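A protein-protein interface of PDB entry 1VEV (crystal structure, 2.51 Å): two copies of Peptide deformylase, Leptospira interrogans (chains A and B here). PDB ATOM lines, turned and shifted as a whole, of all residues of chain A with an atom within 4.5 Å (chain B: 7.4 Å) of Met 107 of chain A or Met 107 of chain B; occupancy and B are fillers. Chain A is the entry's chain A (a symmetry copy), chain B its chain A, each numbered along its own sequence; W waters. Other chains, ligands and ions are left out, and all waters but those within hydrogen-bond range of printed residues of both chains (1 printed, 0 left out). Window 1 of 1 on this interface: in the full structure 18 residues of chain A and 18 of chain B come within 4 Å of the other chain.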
ATOM      1  N   MET A   8      20.858   0.241  13.387  1.00  0.00           N
ATOM      2  CA  MET A   8      20.488  -0.301  12.083  1.00  0.00           C
ATOM      3  C   MET A   8      19.040   0.110  11.808  1.00  0.00           C
ATOM      4  O   MET A   8      18.193   0.086  12.707  1.00  0.00           O
ATOM      5  CB  MET A   8      20.621  -1.824  12.087  1.00  0.00           C
ATOM      6  CG  MET A   8      20.175  -2.484  10.793  1.00  0.00           C
ATOM      7  SD  MET A   8      20.656  -4.217  10.691  1.00  0.00           S
ATOM      8  CE  MET A   8      19.835  -4.891  12.130  1.00  0.00           C
ATOM      9  N   GLU A  99      31.009 -11.672  14.790  1.00  0.00           N
ATOM     10  CA  GLU A  99      31.016 -10.223  14.838  1.00  0.00           C
ATOM     11  C   GLU A  99      29.793  -9.590  15.488  1.00  0.00           C
ATOM     12  O   GLU A  99      28.712 -10.180  15.538  1.00  0.00           O
ATOM     13  CB  GLU A  99      31.166  -9.665  13.425  1.00  0.00           C
ATOM     14  CG  GLU A  99      32.560  -9.780  12.857  1.00  0.00           C
ATOM     15  CD  GLU A  99      32.664  -9.206  11.465  1.00  0.00           C
ATOM     16  OE1 GLU A  99      32.204  -8.066  11.247  1.00  0.00           O
ATOM     17  OE2 GLU A  99      33.214  -9.894  10.587  1.00  0.00           O
ATOM     18  N   GLY A 100      29.997  -8.373  15.981  1.00  0.00           N
ATOM     19  CA  GLY A 100      28.941  -7.591  16.594  1.00  0.00           C
ATOM     20  C   GLY A 100      29.137  -6.172  16.081  1.00  0.00           C
ATOM     21  O   GLY A 100      30.185  -5.869  15.522  1.00  0.00           O
ATOM     22  N   VAL A 104      24.158  -2.290  15.937  1.00  0.00           N
ATOM     23  CA  VAL A 104      23.277  -3.449  15.956  1.00  0.00           C
ATOM     24  C   VAL A 104      23.380  -4.047  17.353  1.00  0.00           C
ATOM     25  O   VAL A 104      23.895  -5.141  17.536  1.00  0.00           O
ATOM     26  CB  VAL A 104      23.722  -4.501  14.926  1.00  0.00           C
ATOM     27  CG1 VAL A 104      22.687  -5.607  14.835  1.00  0.00           C
ATOM     28  CG2 VAL A 104      23.934  -3.846  13.572  1.00  0.00           C
ATOM     29  N   PRO A 105      22.880  -3.319  18.358  1.00  0.00           N
ATOM     30  CA  PRO A 105      22.878  -3.688  19.781  1.00  0.00           C
ATOM     31  C   PRO A 105      22.347  -5.068  20.149  1.00  0.00           C
ATOM     32  O   PRO A 105      21.375  -5.559  19.567  1.00  0.00           O
ATOM     33  CB  PRO A 105      22.027  -2.593  20.425  1.00  0.00           C
ATOM     34  CG  PRO A 105      22.209  -1.421  19.496  1.00  0.00           C
ATOM     35  CD  PRO A 105      22.135  -2.066  18.143  1.00  0.00           C
ATOM     36  N   GLY A 106      22.998  -5.679  21.134  1.00  0.00           N
ATOM     37  CA  GLY A 106      22.578  -6.973  21.647  1.00  0.00           C
ATOM     38  C   GLY A 106      22.657  -8.195  20.761  1.00  0.00           C
ATOM     39  O   GLY A 106      22.161  -9.260  21.135  1.00  0.00           O
ATOM     40  N   MET A 107      23.283  -8.076  19.599  1.00  0.00           N
ATOM     41  CA  MET A 107      23.369  -9.235  18.732  1.00  0.00           C
ATOM     42  C   MET A 107      24.769  -9.582  18.244  1.00  0.00           C
ATOM     43  O   MET A 107      25.718  -8.821  18.416  1.00  0.00           O
ATOM     44  CB  MET A 107      22.419  -9.056  17.554  1.00  0.00           C
ATOM     45  CG  MET A 107      20.965  -8.999  17.980  1.00  0.00           C
ATOM     46  SD  MET A 107      19.925  -8.349  16.677  1.00  0.00           S
ATOM     47  CE  MET A 107      19.588  -9.831  15.812  1.00  0.00           C
ATOM     48  N   ARG A 108      24.875 -10.757  17.640  1.00  0.00           N
ATOM     49  CA  ARG A 108      26.133 -11.256  17.132  1.00  0.00           C
ATOM     50  C   ARG A 108      25.827 -12.187  15.955  1.00  0.00           C
ATOM     51  O   ARG A 108      24.839 -12.920  15.970  1.00  0.00           O
ATOM     52  CB  ARG A 108      26.841 -12.028  18.244  1.00  0.00           C
ATOM     53  CG  ARG A 108      28.340 -11.901  18.235  1.00  0.00           C
ATOM     54  CD  ARG A 108      28.831 -11.092  19.432  1.00  0.00           C
ATOM     55  NE  ARG A 108      28.213  -9.771  19.515  1.00  0.00           N
ATOM     56  CZ  ARG A 108      28.608  -8.818  20.357  1.00  0.00           C
ATOM     57  NH1 ARG A 108      29.622  -9.041  21.184  1.00  0.00           N
ATOM     58  NH2 ARG A 108      27.987  -7.642  20.378  1.00  0.00           N
ATOM     59  N   TYR A 153      27.584  -5.634   9.004  1.00  0.00           N
ATOM     60  CA  TYR A 153      27.947  -7.046   9.036  1.00  0.00           C
ATOM     61  C   TYR A 153      26.799  -8.024   8.780  1.00  0.00           C
ATOM     62  O   TYR A 153      27.029  -9.158   8.350  1.00  0.00           O
ATOM     63  CB  TYR A 153      28.647  -7.378  10.355  1.00  0.00           C
ATOM     64  CG  TYR A 153      27.726  -7.692  11.509  1.00  0.00           C
ATOM     65  CD1 TYR A 153      27.273  -8.993  11.726  1.00  0.00           C
ATOM     66  CD2 TYR A 153      27.322  -6.694  12.396  1.00  0.00           C
ATOM     67  CE1 TYR A 153      26.445  -9.295  12.801  1.00  0.00           C
ATOM     68  CE2 TYR A 153      26.492  -6.983  13.471  1.00  0.00           C
ATOM     69  CZ  TYR A 153      26.058  -8.283  13.669  1.00  0.00           C
ATOM     70  OH  TYR A 153      25.245  -8.577  14.737  1.00  0.00           O
ATOM     71  N   PHE A 163      23.145 -16.518  13.883  1.00  0.00           N
ATOM     72  CA  PHE A 163      22.896 -15.115  14.137  1.00  0.00           C
ATOM     73  C   PHE A 163      21.865 -15.029  15.257  1.00  0.00           C
ATOM     74  O   PHE A 163      20.902 -15.800  15.278  1.00  0.00           O
ATOM     75  CB  PHE A 163      22.365 -14.491  12.847  1.00  0.00           C
ATOM     76  CG  PHE A 163      21.924 -13.068  12.987  1.00  0.00           C
ATOM     77  CD1 PHE A 163      22.760 -12.118  13.564  1.00  0.00           C
ATOM     78  CD2 PHE A 163      20.683 -12.667  12.500  1.00  0.00           C
ATOM     79  CE1 PHE A 163      22.372 -10.790  13.651  1.00  0.00           C
ATOM     80  CE2 PHE A 163      20.282 -11.344  12.579  1.00  0.00           C
ATOM     81  CZ  PHE A 163      21.131 -10.399  13.155  1.00  0.00           C
ATOM     82  N   GLY A 164      22.063 -14.110  16.195  1.00  0.00           N
ATOM     83  CA  GLY A 164      21.117 -13.989  17.287  1.00  0.00           C
ATOM     84  C   GLY A 164      21.501 -13.019  18.386  1.00  0.00           C
ATOM     85  O   GLY A 164      22.385 -12.181  18.210  1.00  0.00           O
ATOM     86  N   PHE A 165      20.822 -13.131  19.524  1.00  0.00           N
ATOM     87  CA  PHE A 165      21.077 -12.263  20.658  1.00  0.00           C
ATOM     88  C   PHE A 165      22.212 -12.811  21.511  1.00  0.00           C
ATOM     89  O   PHE A 165      22.321 -14.024  21.719  1.00  0.00           O
ATOM     90  CB  PHE A 165      19.804 -12.094  21.486  1.00  0.00           C
ATOM     91  CG  PHE A 165      18.698 -11.423  20.736  1.00  0.00           C
ATOM     92  CD1 PHE A 165      17.884 -12.153  19.868  1.00  0.00           C
ATOM     93  CD2 PHE A 165      18.526 -10.044  20.818  1.00  0.00           C
ATOM     94  CE1 PHE A 165      16.919 -11.516  19.084  1.00  0.00           C
ATOM     95  CE2 PHE A 165      17.561  -9.392  20.037  1.00  0.00           C
ATOM     96  CZ  PHE A 165      16.757 -10.132  19.166  1.00  0.00           C
ATOM     97  N   ASN A 166      23.053 -11.899  21.991  1.00  0.00           N
ATOM     98  CA  ASN A 166      24.221 -12.226  22.809  1.00  0.00           C
ATOM     99  C   ASN A 166      23.981 -13.189  23.968  1.00  0.00           C
ATOM    100  O   ASN A 166      24.517 -14.301  23.985  1.00  0.00           O
ATOM    101  CB  ASN A 166      24.823 -10.937  23.355  1.00  0.00           C
ATOM    102  CG  ASN A 166      25.197  -9.969  22.261  1.00  0.00           C
ATOM    103  OD1 ASN A 166      25.527  -8.816  22.529  1.00  0.00           O
ATOM    104  ND2 ASN A 166      25.157 -10.434  21.018  1.00  0.00           N
ATOM    105  N   ARG B   7      14.443 -16.414  22.545  1.00  0.00           N
ATOM    106  CA  ARG B   7      14.941 -15.407  21.609  1.00  0.00           C
ATOM    107  C   ARG B   7      15.800 -16.053  20.543  1.00  0.00           C
ATOM    108  O   ARG B   7      16.392 -17.114  20.765  1.00  0.00           O
ATOM    109  CB  ARG B   7      15.769 -14.351  22.345  1.00  0.00           C
ATOM    110  CG  ARG B   7      14.984 -13.549  23.364  1.00  0.00           C
ATOM    111  CD  ARG B   7      15.783 -13.341  24.645  1.00  0.00           C
ATOM    112  NE  ARG B   7      16.911 -12.430  24.470  1.00  0.00           N
ATOM    113  CZ  ARG B   7      16.784 -11.127  24.235  1.00  0.00           C
ATOM    114  NH1 ARG B   7      15.577 -10.582  24.150  1.00  0.00           N
ATOM    115  NH2 ARG B   7      17.864 -10.367  24.086  1.00  0.00           N
ATOM    116  N   MET B   8      15.863 -15.418  19.377  1.00  0.00           N
ATOM    117  CA  MET B   8      16.686 -15.935  18.289  1.00  0.00           C
ATOM    118  C   MET B   8      18.078 -16.217  18.857  1.00  0.00           C
ATOM    119  O   MET B   8      18.604 -15.439  19.660  1.00  0.00           O
ATOM    120  CB  MET B   8      16.766 -14.913  17.155  1.00  0.00           C
ATOM    121  CG  MET B   8      17.673 -15.333  16.010  1.00  0.00           C
ATOM    122  SD  MET B   8      17.487 -14.291  14.553  1.00  0.00           S
ATOM    123  CE  MET B   8      17.910 -12.685  15.218  1.00  0.00           C
ATOM    124  N   ARG B  70       1.201  -3.508  18.197  1.00  0.00           N
ATOM    125  CA  ARG B  70       2.458  -3.704  17.495  1.00  0.00           C
ATOM    126  C   ARG B  70       2.353  -3.557  15.972  1.00  0.00           C
ATOM    127  O   ARG B  70       3.286  -3.069  15.340  1.00  0.00           O
ATOM    128  CB  ARG B  70       3.043  -5.064  17.871  1.00  0.00           C
ATOM    129  CG  ARG B  70       3.500  -5.142  19.333  1.00  0.00           C
ATOM    130  CD  ARG B  70       4.044  -6.521  19.681  1.00  0.00           C
ATOM    131  NE  ARG B  70       5.051  -6.952  18.718  1.00  0.00           N
ATOM    132  CZ  ARG B  70       5.147  -8.193  18.255  1.00  0.00           C
ATOM    133  NH1 ARG B  70       6.089  -8.514  17.374  1.00  0.00           N
ATOM    134  NH2 ARG B  70       4.292  -9.114  18.678  1.00  0.00           N
ATOM    135  N   TYR B  71       1.233  -3.966  15.382  1.00  0.00           N
ATOM    136  CA  TYR B  71       1.053  -3.837  13.934  1.00  0.00           C
ATOM    137  C   TYR B  71      -0.249  -3.107  13.620  1.00  0.00           C
ATOM    138  O   TYR B  71      -1.239  -3.722  13.237  1.00  0.00           O
ATOM    139  CB  TYR B  71       1.035  -5.206  13.253  1.00  0.00           C
ATOM    140  CG  TYR B  71       2.253  -6.049  13.531  1.00  0.00           C
ATOM    141  CD1 TYR B  71       2.354  -6.785  14.706  1.00  0.00           C
ATOM    142  CD2 TYR B  71       3.319  -6.096  12.628  1.00  0.00           C
ATOM    143  CE1 TYR B  71       3.478  -7.546  14.983  1.00  0.00           C
ATOM    144  CE2 TYR B  71       4.456  -6.857  12.898  1.00  0.00           C
ATOM    145  CZ  TYR B  71       4.525  -7.580  14.082  1.00  0.00           C
ATOM    146  OH  TYR B  71       5.635  -8.341  14.377  1.00  0.00           O
ATOM    147  N   TRP B  98       6.311  -5.688   6.538  1.00  0.00           N
ATOM    148  CA  TRP B  98       7.414  -5.534   7.474  1.00  0.00           C
ATOM    149  C   TRP B  98       7.136  -6.396   8.689  1.00  0.00           C
ATOM    150  O   TRP B  98       6.615  -5.928   9.697  1.00  0.00           O
ATOM    151  CB  TRP B  98       7.583  -4.072   7.889  1.00  0.00           C
ATOM    152  CG  TRP B  98       8.272  -3.263   6.856  1.00  0.00           C
ATOM    153  CD1 TRP B  98       7.707  -2.662   5.776  1.00  0.00           C
ATOM    154  CD2 TRP B  98       9.680  -3.001   6.773  1.00  0.00           C
ATOM    155  NE1 TRP B  98       8.673  -2.036   5.018  1.00  0.00           N
ATOM    156  CE2 TRP B  98       9.893  -2.229   5.609  1.00  0.00           C
ATOM    157  CE3 TRP B  98      10.782  -3.343   7.570  1.00  0.00           C
ATOM    158  CZ2 TRP B  98      11.165  -1.793   5.223  1.00  0.00           C
ATOM    159  CZ3 TRP B  98      12.045  -2.908   7.184  1.00  0.00           C
ATOM    160  CH2 TRP B  98      12.223  -2.141   6.020  1.00  0.00           C
ATOM    161  N   GLU B  99       7.489  -7.668   8.574  1.00  0.00           N
ATOM    162  CA  GLU B  99       7.270  -8.622   9.643  1.00  0.00           C
ATOM    163  C   GLU B  99       8.138  -8.420  10.879  1.00  0.00           C
ATOM    164  O   GLU B  99       9.220  -7.835  10.817  1.00  0.00           O
ATOM    165  CB  GLU B  99       7.487 -10.040   9.117  1.00  0.00           C
ATOM    166  CG  GLU B  99       6.364 -10.559   8.253  1.00  0.00           C
ATOM    167  CD  GLU B  99       6.615 -11.965   7.766  1.00  0.00           C
ATOM    168  OE1 GLU B  99       6.960 -12.836   8.591  1.00  0.00           O
ATOM    169  OE2 GLU B  99       6.459 -12.202   6.555  1.00  0.00           O
ATOM    170  N   GLY B 100       7.629  -8.923  11.999  1.00  0.00           N
ATOM    171  CA  GLY B 100       8.329  -8.872  13.267  1.00  0.00           C
ATOM    172  C   GLY B 100       8.109 -10.235  13.908  1.00  0.00           C
ATOM    173  O   GLY B 100       7.253 -10.986  13.455  1.00  0.00           O
ATOM    174  N   CYS B 101       8.868 -10.574  14.942  1.00  0.00           N
ATOM    175  CA  CYS B 101       8.707 -11.867  15.602  1.00  0.00           C
ATOM    176  C   CYS B 101       8.993 -11.726  17.092  1.00  0.00           C
ATOM    177  O   CYS B 101       9.967 -11.097  17.480  1.00  0.00           O
ATOM    178  CB  CYS B 101       9.651 -12.897  14.980  1.00  0.00           C
ATOM    179  SG  CYS B 101       9.708 -14.489  15.840  1.00  0.00           S
ATOM    180  N   VAL B 104      12.316 -12.308  18.137  1.00  0.00           N
ATOM    181  CA  VAL B 104      13.298 -11.384  17.585  1.00  0.00           C
ATOM    182  C   VAL B 104      12.854  -9.987  17.995  1.00  0.00           C
ATOM    183  O   VAL B 104      12.461  -9.179  17.164  1.00  0.00           O
ATOM    184  CB  VAL B 104      13.338 -11.469  16.049  1.00  0.00           C
ATOM    185  CG1 VAL B 104      14.491 -10.639  15.515  1.00  0.00           C
ATOM    186  CG2 VAL B 104      13.464 -12.918  15.611  1.00  0.00           C
ATOM    187  N   PRO B 105      12.917  -9.692  19.298  1.00  0.00           N
ATOM    188  CA  PRO B 105      12.534  -8.417  19.921  1.00  0.00           C
ATOM    189  C   PRO B 105      13.108  -7.140  19.321  1.00  0.00           C
ATOM    190  O   PRO B 105      14.269  -7.092  18.904  1.00  0.00           O
ATOM    191  CB  PRO B 105      12.989  -8.586  21.371  1.00  0.00           C
ATOM    192  CG  PRO B 105      12.943 -10.076  21.578  1.00  0.00           C
ATOM    193  CD  PRO B 105      13.515 -10.600  20.294  1.00  0.00           C
ATOM    194  N   GLY B 106      12.275  -6.104  19.297  1.00  0.00           N
ATOM    195  CA  GLY B 106      12.689  -4.796  18.814  1.00  0.00           C
ATOM    196  C   GLY B 106      13.053  -4.611  17.359  1.00  0.00           C
ATOM    197  O   GLY B 106      13.550  -3.548  16.978  1.00  0.00           O
ATOM    198  N   MET B 107      12.803  -5.612  16.528  1.00  0.00           N
ATOM    199  CA  MET B 107      13.146  -5.458  15.128  1.00  0.00           C
ATOM    200  C   MET B 107      12.024  -5.762  14.145  1.00  0.00           C
ATOM    201  O   MET B 107      10.974  -6.286  14.508  1.00  0.00           O
ATOM    202  CB  MET B 107      14.377  -6.297  14.813  1.00  0.00           C
ATOM    203  CG  MET B 107      15.609  -5.832  15.566  1.00  0.00           C
ATOM    204  SD  MET B 107      16.900  -7.071  15.540  1.00  0.00           S
ATOM    205  CE  MET B 107      17.685  -6.637  14.038  1.00  0.00           C
ATOM    206  N   ARG B 108      12.269  -5.410  12.891  1.00  0.00           N
ATOM    207  CA  ARG B 108      11.308  -5.606  11.829  1.00  0.00           C
ATOM    208  C   ARG B 108      12.083  -5.776  10.519  1.00  0.00           C
ATOM    209  O   ARG B 108      13.109  -5.131  10.304  1.00  0.00           O
ATOM    210  CB  ARG B 108      10.404  -4.376  11.750  1.00  0.00           C
ATOM    211  CG  ARG B 108       8.977  -4.673  11.376  1.00  0.00           C
ATOM    212  CD  ARG B 108       8.038  -4.431  12.554  1.00  0.00           C
ATOM    213  NE  ARG B 108       8.415  -5.187  13.745  1.00  0.00           N
ATOM    214  CZ  ARG B 108       7.655  -5.285  14.834  1.00  0.00           C
ATOM    215  NH1 ARG B 108       6.476  -4.676  14.879  1.00  0.00           N
ATOM    216  NH2 ARG B 108       8.074  -5.987  15.883  1.00  0.00           N
ATOM    217  N   GLY B 109      11.600  -6.652   9.649  1.00  0.00           N
ATOM    218  CA  GLY B 109      12.275  -6.870   8.382  1.00  0.00           C
ATOM    219  C   GLY B 109      11.269  -7.098   7.276  1.00  0.00           C
ATOM    220  O   GLY B 109      10.223  -7.695   7.503  1.00  0.00           O
ATOM    221  N   TYR B 153      11.670 -15.479  10.357  1.00  0.00           N
ATOM    222  CA  TYR B 153      11.510 -14.543   9.250  1.00  0.00           C
ATOM    223  C   TYR B 153      12.803 -13.905   8.740  1.00  0.00           C
ATOM    224  O   TYR B 153      12.872 -13.472   7.586  1.00  0.00           O
ATOM    225  CB  TYR B 153      10.491 -13.463   9.620  1.00  0.00           C
ATOM    226  CG  TYR B 153      11.048 -12.294  10.396  1.00  0.00           C
ATOM    227  CD1 TYR B 153      11.584 -11.190   9.735  1.00  0.00           C
ATOM    228  CD2 TYR B 153      11.020 -12.282  11.791  1.00  0.00           C
ATOM    229  CE1 TYR B 153      12.076 -10.099  10.443  1.00  0.00           C
ATOM    230  CE2 TYR B 153      11.512 -11.199  12.508  1.00  0.00           C
ATOM    231  CZ  TYR B 153      12.036 -10.112  11.830  1.00  0.00           C
ATOM    232  OH  TYR B 153      12.515  -9.034  12.534  1.00  0.00           O
ATOM    233  N   VAL B 154      13.828 -13.849   9.582  1.00  0.00           N
ATOM    234  CA  VAL B 154      15.088 -13.257   9.157  1.00  0.00           C
ATOM    235  C   VAL B 154      15.742 -14.124   8.085  1.00  0.00           C
ATOM    236  O   VAL B 154      16.593 -13.658   7.330  1.00  0.00           O
ATOM    237  CB  VAL B 154      16.063 -13.082  10.348  1.00  0.00           C
ATOM    238  CG1 VAL B 154      15.382 -12.287  11.462  1.00  0.00           C
ATOM    239  CG2 VAL B 154      16.520 -14.440  10.856  1.00  0.00           C
ATOM    240  N   PHE B 163      15.833  -3.950   6.936  1.00  0.00           N
ATOM    241  CA  PHE B 163      15.800  -4.690   8.180  1.00  0.00           C
ATOM    242  C   PHE B 163      16.416  -3.802   9.256  1.00  0.00           C
ATOM    243  O   PHE B 163      17.421  -3.131   9.010  1.00  0.00           O
ATOM    244  CB  PHE B 163      16.611  -5.971   7.987  1.00  0.00           C
ATOM    245  CG  PHE B 163      16.790  -6.779   9.232  1.00  0.00           C
ATOM    246  CD1 PHE B 163      15.697  -7.125  10.019  1.00  0.00           C
ATOM    247  CD2 PHE B 163      18.054  -7.234   9.597  1.00  0.00           C
ATOM    248  CE1 PHE B 163      15.855  -7.915  11.147  1.00  0.00           C
ATOM    249  CE2 PHE B 163      18.228  -8.025  10.721  1.00  0.00           C
ATOM    250  CZ  PHE B 163      17.122  -8.370  11.499  1.00  0.00           C
ATOM    251  N   GLY B 164      15.816  -3.782  10.441  1.00  0.00           N
ATOM    252  CA  GLY B 164      16.356  -2.950  11.500  1.00  0.00           C
ATOM    253  C   GLY B 164      15.526  -2.874  12.765  1.00  0.00           C
ATOM    254  O   GLY B 164      14.633  -3.691  12.986  1.00  0.00           O
ATOM    255  N   PHE B 165      15.832  -1.886  13.602  1.00  0.00           N
ATOM    256  CA  PHE B 165      15.125  -1.697  14.854  1.00  0.00           C
ATOM    257  C   PHE B 165      13.869  -0.865  14.645  1.00  0.00           C
ATOM    258  O   PHE B 165      13.867   0.097  13.868  1.00  0.00           O
ATOM    259  CB  PHE B 165      16.048  -1.044  15.883  1.00  0.00           C
ATOM    260  CG  PHE B 165      17.229  -1.890  16.237  1.00  0.00           C
ATOM    261  CD1 PHE B 165      18.361  -1.906  15.421  1.00  0.00           C
ATOM    262  CD2 PHE B 165      17.179  -2.748  17.332  1.00  0.00           C
ATOM    263  CE1 PHE B 165      19.424  -2.773  15.686  1.00  0.00           C
ATOM    264  CE2 PHE B 165      18.239  -3.623  17.610  1.00  0.00           C
ATOM    265  CZ  PHE B 165      19.363  -3.636  16.782  1.00  0.00           C
ATOM    266  N   ASN B 166      12.806  -1.255  15.342  1.00  0.00           N
ATOM    267  CA  ASN B 166      11.499  -0.603  15.258  1.00  0.00           C
ATOM    268  C   ASN B 166      11.500   0.919  15.362  1.00  0.00           C
ATOM    269  O   ASN B 166      11.141   1.616  14.409  1.00  0.00           O
ATOM    270  CB  ASN B 166      10.589  -1.171  16.341  1.00  0.00           C
ATOM    271  CG  ASN B 166      10.441  -2.668  16.240  1.00  0.00           C
ATOM    272  OD1 ASN B 166       9.891  -3.307  17.135  1.00  0.00           O
ATOM    273  ND2 ASN B 166      10.923  -3.239  15.143  1.00  0.00           N
ATOM    274  N   GLU B 167      11.887   1.423  16.531  1.00  0.00           N
ATOM    275  CA  GLU B 167      11.928   2.859  16.784  1.00  0.00           C
ATOM    276  C   GLU B 167      12.659   3.611  15.675  1.00  0.00           C
ATOM    277  O   GLU B 167      12.317   4.749  15.349  1.00  0.00           O
ATOM    278  CB  GLU B 167      12.595   3.132  18.134  1.00  0.00           C
ATOM    279  N   LEU B 169      13.221   2.332  12.341  1.00  0.00           N
ATOM    280  CA  LEU B 169      12.496   2.136  11.090  1.00  0.00           C
ATOM    281  C   LEU B 169      11.342   3.131  11.010  1.00  0.00           C
ATOM    282  O   LEU B 169      11.095   3.739   9.963  1.00  0.00           O
ATOM    283  CB  LEU B 169      11.956   0.706  11.031  1.00  0.00           C
ATOM    284  CG  LEU B 169      12.746  -0.355  10.261  1.00  0.00           C
ATOM    285  CD1 LEU B 169      14.229  -0.090  10.336  1.00  0.00           C
ATOM    286  CD2 LEU B 169      12.406  -1.721  10.828  1.00  0.00           C
HETATM  287  O   HOH W   1      20.360  -8.835  23.917  1.00  0.00           O
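Among the printed residues, pairs that only touch across the chains: Phe 163 of chain A with Met 8 of chain B (3.3 Å), Met 8 of chain A with Phe 163 of chain B (3.3 Å), Phe 165 of chain A with Arg 7 of chain B (3.3 Å), Met 8 of chain A with Met 107 of chain B (3.4 Å), Met 107 of chain A with Met 8 of chain B (3.4 Å), Pro 105 of chain A with Phe 165 of chain B (3.5 Å), Phe 165 of chain A with Pro 105 of chain B (3.5 Å), Met 8 of chain A with Gly 164 of chain B (3.7 Å), Gly 164 of chain A with Met 8 of chain B (3.7 Å), Val 104 of chain A with Phe 165 of chain B (3.9 Å) and Phe 165 of chain A with Val 104 of chain B (3.9 Å).
Met 8 of chain A touches Met 107 of chain B, and with the chains exchanged Met 107 of chain A touches Met 8 of chain B. Met 8 of chain A touches Phe 163 of chain B, and with the chains exchanged Phe 163 of chain A touches Met 8 of chain B. Met 8 of chain A touches Phe 165 of chain B, and with the chains exchanged Phe 165 of chain A touches Met 8 of chain B. Met 107 of chain A touches its own counterpart, Met 107 of chain B. 13 positions are printed for both chains.
Of the 13 printed residues of chain A, 7 touch a printed residue of chain B. Hydrophobic or aromatic side chains of chain B within 4 Å of the printed part of chain A: Met 8, Pro 105, Met 107, Phe 163 and Phe 165. Among the printed residues, 14 pairs touch across the chains. Among the printed residues, no Asp or Glu carboxylate lies within 4 Å of a Lys or Arg side-chain nitrogen of the other chain.
Of chain B, only Met 8 and Met 107 come within 4 Å of Met 107 of chain A. No residue of chain B comes within 4 Å of Gly 106 of chain A. Of the printed residues of chain A, Phe 165 of chain B touches Met 8 (3.2 Å), Val 104 (3.9 Å) and Pro 105 (3.5 Å). Of the printed residues of chain A, Pro 105 of chain B touches Phe 165 (3.5 Å). Printed residues of chain A within 4 Å of Arg 7 of chain B: Phe 165. Of the printed residues of chain B, Phe 165 of chain A touches Arg 7 (3.3 Å), Met 8 (3.2 Å), Val 104 (3.9 Å) and Pro 105 (3.5 Å).
O of Met 107 of chain B lies close to ND2 of Asn 166 of chain B. O of Gly 164 of chain B lies within hydrogen-bond range of N of Arg 108 of chain B, 2.9 Å away. The side-chain amide nitrogen (ND2) of Asn 166 of chain A sits close to the backbone carbonyl oxygen (O) of Met 107 of chain A. The backbone carbonyl oxygen (O) of Gly 164 of chain A is in hydrogen-bond range of the backbone NH (N) of Arg 108 of chain A.
Water W1 bridges the guanidinium group of Arg 7 of chain B (2.9 Å) and the backbone carbonyl oxygen of Gly 106 of chain A (3.3 Å).
The backbone carbonyl oxygen (O) of Met 8 of chain B sits at hydrogen-bond distance from the backbone NH (N) of Phe 165 of chain A (3.2 Å). The side-chain sulfur of Met 107 of chain B lies close to the side-chain sulfur of Met 107 of chain A. N of Phe 165 of chain B is in hydrogen-bond range of O of Met 8 of chain A.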
